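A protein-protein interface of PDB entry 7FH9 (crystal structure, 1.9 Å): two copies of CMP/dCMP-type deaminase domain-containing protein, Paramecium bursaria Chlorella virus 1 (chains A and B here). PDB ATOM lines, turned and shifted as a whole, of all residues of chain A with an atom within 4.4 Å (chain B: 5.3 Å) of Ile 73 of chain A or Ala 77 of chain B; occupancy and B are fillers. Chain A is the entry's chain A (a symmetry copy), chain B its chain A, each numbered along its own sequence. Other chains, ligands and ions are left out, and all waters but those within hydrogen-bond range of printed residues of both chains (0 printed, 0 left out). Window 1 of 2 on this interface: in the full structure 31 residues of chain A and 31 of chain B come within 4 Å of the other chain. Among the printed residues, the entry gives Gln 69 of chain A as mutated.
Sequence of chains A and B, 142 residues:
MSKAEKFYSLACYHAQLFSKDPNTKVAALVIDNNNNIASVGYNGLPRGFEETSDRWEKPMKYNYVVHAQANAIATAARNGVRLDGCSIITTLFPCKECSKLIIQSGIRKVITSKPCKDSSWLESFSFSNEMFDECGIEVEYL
The backbone carbonyl oxygen of Ala 77 of chain B sits at hydrogen-bond distance from the backbone NH of Leu 83 of chain A, 2.8 Å away. The backbone carbonyl oxygen (O) of Ala 77 of chain A lies close to the backbone carbonyl oxygen (O) of Val 81 of chain B (3.2 Å). The backbone carbonyl oxygen (O) of Ala 77 of chain B sits close to the backbone carbonyl oxygen (O) of Val 81 of chain A, at 3.2 Å.
Ile 73 of chain A touches Ala 77 of chain B. Ile 73 of chain B touches Ala 77 of chain A. CA of Gly 80 of chain B touches C of Val 81 of chain A (3.7 Å). Ala 77 of chain B touches Arg 82 of chain A (O to CA, 3.5 Å). Arg 82 of chain A touches Arg 78 of chain B (CG to O, 3.3 Å). Gly 80 of chain B touches Arg 82 of chain A. N of Leu 83 of chain A touches O of Arg 78 of chain B, 3.97 Å away. Ser 105 of chain A touches Ala 74 of chain B (CA to O, 3.6 Å). Arg 78 of chain B touches Ser 105 of chain A.
The backbone NH (N) of Val 81 of chain B sits at hydrogen-bond distance from the backbone carbonyl oxygen (O) of Ala 76 of chain B (2.9 Å). N of Val 81 of chain A sits at hydrogen-bond distance from O of Ala 76 of chain A, 2.9 Å away. OG of Ser 105 of chain A is in hydrogen-bond range of O of Leu 101 of chain A (3.4 Å). O of Ile 102 of chain A is in hydrogen-bond range of OG of Ser 105 of chain A.
Of the 9 printed residues of chain B, 6 touch a printed residue of chain A. Printed residues of chain B that touch a printed residue of chain A: Ile 73, Ala 74, Ala 77, Arg 78, Gly 80 and Val 81. Hydrophobic or aromatic side chains of chain B within 4 Å of the printed part of chain A: Ile 73 and Ala 77. Among the printed residues, 12 pairs touch across the chains. Among the printed residues, no Asp or Glu carboxylate lies within 4 Å of a Lys or Arg side-chain nitrogen of the other chain.
Ile 73 of chain A touches Ala 77 of chain B, and with the chains exchanged Ala 77 of chain A touches Ile 73 of chain B. Ala 77 of chain A touches Val 81 of chain B, and with the chains exchanged Val 81 of chain A touches Ala 77 of chain B. Of the 12 pairs that touch across the chains among the printed residues, 4 have their exchanged pair printed and touching as well.
Ile 73 of chain A touches just one residue of chain B: Ala 77. Ala 77 of chain B touches four residues of chain A. Of the printed residues of chain B, Arg 82 of chain A touches Ala 77, Arg 78 and Gly 80. Of the printed residues of chain A, Val 81 of chain B touches Ala 77. Printed residues of chain B within 4 Å of Leu 83 of chain A: Ala 77 (2.8 Å) and Arg 78 (3.97 Å). Of the printed residues of chain A, Ile 73 of chain B touches Ala 77 (3.5 Å). Of the printed residues of chain A, Gly 80 of chain B touches Val 81 (3.7 Å) and Arg 82 (3.6 Å). Thr 75 of chain A touches none of the printed residues of chain B. The nearest residue of chain B that does not touch Ile 73 of chain A is Ala 74 of chain B (4.05 Å). The nearest residue of chain A that does not touch Ala 77 of chain B is Ala 77 of chain A (4.02 Å). The nearest printed residue of chain A that does not touch Gly 80 of chain B is Leu 83 of chain A (5.0 Å).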
ATOM      1  N   GLN A  69      10.160 -20.530   8.160  1.00  0.00           N
ATOM      2  CA  GLN A  69       9.910 -20.005   6.820  1.00  0.00           C
ATOM      3  C   GLN A  69       8.417 -19.974   6.513  1.00  0.00           C
ATOM      4  O   GLN A  69       7.913 -18.978   5.983  1.00  0.00           O
ATOM      5  CB  GLN A  69      10.723 -20.806   5.785  1.00  0.00           C
ATOM      6  CG  GLN A  69      12.233 -20.536   6.007  1.00  0.00           C
ATOM      7  CD  GLN A  69      13.176 -21.339   5.125  1.00  0.00           C
ATOM      8  OE1 GLN A  69      13.350 -21.040   3.940  1.00  0.00           O
ATOM      9  NE2 GLN A  69      13.828 -22.332   5.718  1.00  0.00           N
ATOM     10  N   ALA A  70       7.685 -21.032   6.881  1.00  0.00           N
ATOM     11  CA  ALA A  70       6.224 -20.976   6.838  1.00  0.00           C
ATOM     12  C   ALA A  70       5.682 -19.777   7.607  1.00  0.00           C
ATOM     13  O   ALA A  70       4.776 -19.082   7.125  1.00  0.00           O
ATOM     14  CB  ALA A  70       5.622 -22.264   7.407  1.00  0.00           C
ATOM     15  N   ASN A  71       6.219 -19.524   8.818  1.00  0.00           N
ATOM     16  CA  ASN A  71       5.742 -18.398   9.621  1.00  0.00           C
ATOM     17  C   ASN A  71       5.984 -17.067   8.924  1.00  0.00           C
ATOM     18  O   ASN A  71       5.154 -16.158   9.017  1.00  0.00           O
ATOM     19  CB  ASN A  71       6.415 -18.387  10.995  1.00  0.00           C
ATOM     20  CG  ASN A  71       5.432 -18.641  12.123  1.00  0.00           C
ATOM     21  OD1 ASN A  71       4.236 -18.373  11.988  1.00  0.00           O
ATOM     22  ND2 ASN A  71       5.931 -19.136  13.252  1.00  0.00           N
ATOM     23  N   ALA A  72       7.133 -16.917   8.252  1.00  0.00           N
ATOM     24  CA  ALA A  72       7.414 -15.664   7.553  1.00  0.00           C
ATOM     25  C   ALA A  72       6.363 -15.397   6.489  1.00  0.00           C
ATOM     26  O   ALA A  72       5.953 -14.248   6.271  1.00  0.00           O
ATOM     27  CB  ALA A  72       8.806 -15.715   6.922  1.00  0.00           C
ATOM     28  N   ILE A  73       5.921 -16.454   5.811  1.00  0.00           N
ATOM     29  CA  ILE A  73       4.949 -16.306   4.736  1.00  0.00           C
ATOM     30  C   ILE A  73       3.561 -16.046   5.309  1.00  0.00           C
ATOM     31  O   ILE A  73       2.838 -15.159   4.841  1.00  0.00           O
ATOM     32  CB  ILE A  73       4.976 -17.560   3.838  1.00  0.00           C
ATOM     33  CG1 ILE A  73       6.310 -17.623   3.076  1.00  0.00           C
ATOM     34  CG2 ILE A  73       3.793 -17.565   2.889  1.00  0.00           C
ATOM     35  CD1 ILE A  73       6.646 -18.989   2.523  1.00  0.00           C
ATOM     36  N   ALA A  74       3.160 -16.832   6.311  1.00  0.00           N
ATOM     37  CA  ALA A  74       1.859 -16.621   6.937  1.00  0.00           C
ATOM     38  C   ALA A  74       1.780 -15.251   7.601  1.00  0.00           C
ATOM     39  O   ALA A  74       0.725 -14.610   7.594  1.00  0.00           O
ATOM     40  CB  ALA A  74       1.581 -17.728   7.949  1.00  0.00           C
ATOM     41  N   THR A  75       2.885 -14.786   8.188  1.00  0.00           N
ATOM     42  CA  THR A  75       2.889 -13.461   8.806  1.00  0.00           C
ATOM     43  C   THR A  75       2.715 -12.369   7.753  1.00  0.00           C
ATOM     44  O   THR A  75       2.028 -11.365   7.993  1.00  0.00           O
ATOM     45  CB  THR A  75       4.187 -13.273   9.600  1.00  0.00           C
ATOM     46  OG1 THR A  75       4.231 -14.242  10.661  1.00  0.00           O
ATOM     47  CG2 THR A  75       4.286 -11.865  10.181  1.00  0.00           C
ATOM     48  N   ALA A  76       3.311 -12.551   6.569  1.00  0.00           N
ATOM     49  CA  ALA A  76       3.121 -11.567   5.506  1.00  0.00           C
ATOM     50  C   ALA A  76       1.666 -11.524   5.053  1.00  0.00           C
ATOM     51  O   ALA A  76       1.124 -10.447   4.777  1.00  0.00           O
ATOM     52  CB  ALA A  76       4.046 -11.874   4.322  1.00  0.00           C
ATOM     53  N   ALA A  77       1.014 -12.690   4.975  1.00  0.00           N
ATOM     54  CA  ALA A  77      -0.407 -12.705   4.624  1.00  0.00           C
ATOM     55  C   ALA A  77      -1.238 -11.976   5.676  1.00  0.00           C
ATOM     56  O   ALA A  77      -2.140 -11.197   5.337  1.00  0.00           O
ATOM     57  CB  ALA A  77      -0.895 -14.147   4.455  1.00  0.00           C
ATOM     58  N   VAL A  81       1.648  -7.953   3.297  1.00  0.00           N
ATOM     59  CA  VAL A  81       2.923  -7.535   2.718  1.00  0.00           C
ATOM     60  C   VAL A  81       3.211  -8.420   1.510  1.00  0.00           C
ATOM     61  O   VAL A  81       3.148  -9.649   1.612  1.00  0.00           O
ATOM     62  CB  VAL A  81       4.050  -7.622   3.762  1.00  0.00           C
ATOM     63  CG1 VAL A  81       5.398  -7.330   3.131  1.00  0.00           C
ATOM     64  CG2 VAL A  81       3.775  -6.633   4.917  1.00  0.00           C
ATOM     65  N   ARG A  82       3.504  -7.798   0.365  1.00  0.00           N
ATOM     66  CA  ARG A  82       3.705  -8.522  -0.892  1.00  0.00           C
ATOM     67  C   ARG A  82       5.084  -9.178  -0.918  1.00  0.00           C
ATOM     68  O   ARG A  82       6.106  -8.490  -0.810  1.00  0.00           O
ATOM     69  CB  ARG A  82       3.543  -7.559  -2.066  1.00  0.00           C
ATOM     70  CG  ARG A  82       3.680  -8.186  -3.456  1.00  0.00           C
ATOM     71  CD  ARG A  82       3.901  -7.103  -4.496  1.00  0.00           C
ATOM     72  NE  ARG A  82       4.129  -7.620  -5.839  1.00  0.00           N
ATOM     73  CZ  ARG A  82       5.270  -7.466  -6.511  1.00  0.00           C
ATOM     74  NH1 ARG A  82       6.283  -6.813  -5.956  1.00  0.00           N
ATOM     75  NH2 ARG A  82       5.413  -7.970  -7.738  1.00  0.00           N
ATOM     76  N   LEU A  83       5.117 -10.506  -1.064  1.00  0.00           N
ATOM     77  CA  LEU A  83       6.386 -11.226  -1.111  1.00  0.00           C
ATOM     78  C   LEU A  83       6.834 -11.579  -2.529  1.00  0.00           C
ATOM     79  O   LEU A  83       7.961 -12.059  -2.696  1.00  0.00           O
ATOM     80  CB  LEU A  83       6.315 -12.512  -0.258  1.00  0.00           C
ATOM     81  CG  LEU A  83       5.938 -12.343   1.230  1.00  0.00           C
ATOM     82  CD1 LEU A  83       6.223 -13.631   2.027  1.00  0.00           C
ATOM     83  CD2 LEU A  83       6.610 -11.128   1.889  1.00  0.00           C
ATOM     84  N   LEU A 101       5.691 -23.707  -0.089  1.00  0.00           N
ATOM     85  CA  LEU A 101       5.089 -22.424   0.277  1.00  0.00           C
ATOM     86  C   LEU A 101       5.939 -21.261  -0.211  1.00  0.00           C
ATOM     87  O   LEU A 101       5.407 -20.210  -0.587  1.00  0.00           O
ATOM     88  CB  LEU A 101       4.905 -22.326   1.790  1.00  0.00           C
ATOM     89  CG  LEU A 101       4.021 -23.414   2.406  1.00  0.00           C
ATOM     90  CD1 LEU A 101       3.978 -23.241   3.904  1.00  0.00           C
ATOM     91  CD2 LEU A 101       2.612 -23.399   1.808  1.00  0.00           C
ATOM     92  N   ILE A 102       7.263 -21.427  -0.178  1.00  0.00           N
ATOM     93  CA  ILE A 102       8.166 -20.409  -0.715  1.00  0.00           C
ATOM     94  C   ILE A 102       7.850 -20.145  -2.182  1.00  0.00           C
ATOM     95  O   ILE A 102       7.761 -18.991  -2.621  1.00  0.00           O
ATOM     96  CB  ILE A 102       9.631 -20.839  -0.519  1.00  0.00           C
ATOM     97  CG1 ILE A 102      10.030 -20.692   0.951  1.00  0.00           C
ATOM     98  CG2 ILE A 102      10.574 -20.029  -1.457  1.00  0.00           C
ATOM     99  CD1 ILE A 102      11.317 -21.402   1.303  1.00  0.00           C
ATOM    100  N   SER A 105       4.443 -18.338  -2.531  1.00  0.00           N
ATOM    101  CA  SER A 105       4.462 -16.947  -2.089  1.00  0.00           C
ATOM    102  C   SER A 105       5.171 -16.015  -3.065  1.00  0.00           C
ATOM    103  O   SER A 105       5.203 -14.808  -2.826  1.00  0.00           O
ATOM    104  CB  SER A 105       5.131 -16.847  -0.712  1.00  0.00           C
ATOM    105  OG  SER A 105       6.523 -17.058  -0.841  1.00  0.00           O
ATOM    106  N   ILE A 107       8.412 -15.860  -3.679  1.00  0.00           N
ATOM    107  CA  ILE A 107       9.832 -15.693  -3.383  1.00  0.00           C
ATOM    108  C   ILE A 107      10.675 -16.320  -4.494  1.00  0.00           C
ATOM    109  O   ILE A 107      10.388 -17.420  -4.977  1.00  0.00           O
ATOM    110  CB  ILE A 107      10.134 -16.303  -2.001  1.00  0.00           C
ATOM    111  CG1 ILE A 107       9.504 -15.441  -0.904  1.00  0.00           C
ATOM    112  CG2 ILE A 107      11.637 -16.471  -1.764  1.00  0.00           C
ATOM    113  CD1 ILE A 107       9.456 -16.099   0.488  1.00  0.00           C
ATOM    114  N   ILE B  73      -3.403 -18.930   1.771  1.00  0.00           N
ATOM    115  CA  ILE B  73      -2.600 -18.046   2.605  1.00  0.00           C
ATOM    116  C   ILE B  73      -1.321 -17.649   1.879  1.00  0.00           C
ATOM    117  O   ILE B  73      -0.938 -16.473   1.867  1.00  0.00           O
ATOM    118  CB  ILE B  73      -2.308 -18.733   3.954  1.00  0.00           C
ATOM    119  CG1 ILE B  73      -3.610 -18.864   4.762  1.00  0.00           C
ATOM    120  CG2 ILE B  73      -1.250 -17.968   4.727  1.00  0.00           C
ATOM    121  CD1 ILE B  73      -3.551 -19.891   5.871  1.00  0.00           C
ATOM    122  N   ALA B  74      -0.630 -18.625   1.287  1.00  0.00           N
ATOM    123  CA  ALA B  74       0.586 -18.319   0.541  1.00  0.00           C
ATOM    124  C   ALA B  74       0.291 -17.416  -0.652  1.00  0.00           C
ATOM    125  O   ALA B  74       1.097 -16.547  -0.997  1.00  0.00           O
ATOM    126  CB  ALA B  74       1.259 -19.610   0.087  1.00  0.00           C
ATOM    127  N   THR B  75      -0.859 -17.611  -1.303  1.00  0.00           N
ATOM    128  CA  THR B  75      -1.223 -16.752  -2.427  1.00  0.00           C
ATOM    129  C   THR B  75      -1.465 -15.318  -1.962  1.00  0.00           C
ATOM    130  O   THR B  75      -1.101 -14.359  -2.659  1.00  0.00           O
ATOM    131  CB  THR B  75      -2.457 -17.330  -3.131  1.00  0.00           C
ATOM    132  OG1 THR B  75      -2.127 -18.623  -3.666  1.00  0.00           O
ATOM    133  CG2 THR B  75      -2.938 -16.413  -4.254  1.00  0.00           C
ATOM    134  N   ALA B  76      -2.060 -15.145  -0.777  1.00  0.00           N
ATOM    135  CA  ALA B  76      -2.254 -13.793  -0.258  1.00  0.00           C
ATOM    136  C   ALA B  76      -0.918 -13.119   0.029  1.00  0.00           C
ATOM    137  O   ALA B  76      -0.751 -11.919  -0.225  1.00  0.00           O
ATOM    138  CB  ALA B  76      -3.123 -13.827   1.006  1.00  0.00           C
ATOM    139  N   ALA B  77       0.051 -13.877   0.554  1.00  0.00           N
ATOM    140  CA  ALA B  77       1.381 -13.306   0.775  1.00  0.00           C
ATOM    141  C   ALA B  77       2.023 -12.886  -0.544  1.00  0.00           C
ATOM    142  O   ALA B  77       2.618 -11.803  -0.637  1.00  0.00           O
ATOM    143  CB  ALA B  77       2.272 -14.310   1.514  1.00  0.00           C
ATOM    144  N   ARG B  78       1.897 -13.720  -1.583  1.00  0.00           N
ATOM    145  CA  ARG B  78       2.396 -13.334  -2.905  1.00  0.00           C
ATOM    146  C   ARG B  78       1.756 -12.037  -3.390  1.00  0.00           C
ATOM    147  O   ARG B  78       2.442 -11.158  -3.931  1.00  0.00           O
ATOM    148  CB  ARG B  78       2.136 -14.445  -3.926  1.00  0.00           C
ATOM    149  CG  ARG B  78       2.726 -14.108  -5.312  1.00  0.00           C
ATOM    150  CD  ARG B  78       2.454 -15.192  -6.340  1.00  0.00           C
ATOM    151  NE  ARG B  78       3.155 -14.908  -7.595  1.00  0.00           N
ATOM    152  CZ  ARG B  78       2.711 -15.254  -8.798  1.00  0.00           C
ATOM    153  NH1 ARG B  78       1.556 -15.884  -8.930  1.00  0.00           N
ATOM    154  NH2 ARG B  78       3.422 -14.957  -9.876  1.00  0.00           N
ATOM    155  N   ASN B  79       0.433 -11.916  -3.245  1.00  0.00           N
ATOM    156  CA  ASN B  79      -0.280 -10.751  -3.757  1.00  0.00           C
ATOM    157  C   ASN B  79      -0.276  -9.573  -2.795  1.00  0.00           C
ATOM    158  O   ASN B  79      -0.704  -8.481  -3.184  1.00  0.00           O
ATOM    159  CB  ASN B  79      -1.737 -11.103  -4.085  1.00  0.00           C
ATOM    160  CG  ASN B  79      -1.861 -12.204  -5.101  1.00  0.00           C
ATOM    161  OD1 ASN B  79      -2.713 -13.093  -4.977  1.00  0.00           O
ATOM    162  ND2 ASN B  79      -1.016 -12.163  -6.116  1.00  0.00           N
ATOM    163  N   GLY B  80       0.182  -9.762  -1.564  1.00  0.00           N
ATOM    164  CA  GLY B  80       0.147  -8.694  -0.576  1.00  0.00           C
ATOM    165  C   GLY B  80      -1.253  -8.330  -0.128  1.00  0.00           C
ATOM    166  O   GLY B  80      -1.558  -7.141   0.033  1.00  0.00           O
ATOM    167  N   VAL B  81      -2.114  -9.323   0.071  1.00  0.00           N
ATOM    168  CA  VAL B  81      -3.493  -9.108   0.503  1.00  0.00           C
ATOM    169  C   VAL B  81      -3.582  -9.428   1.991  1.00  0.00           C
ATOM    170  O   VAL B  81      -3.141 -10.497   2.424  1.00  0.00           O
ATOM    171  CB  VAL B  81      -4.463  -9.974  -0.321  1.00  0.00           C
ATOM    172  CG1 VAL B  81      -5.878  -9.865   0.218  1.00  0.00           C
ATOM    173  CG2 VAL B  81      -4.421  -9.547  -1.804  1.00  0.00           C
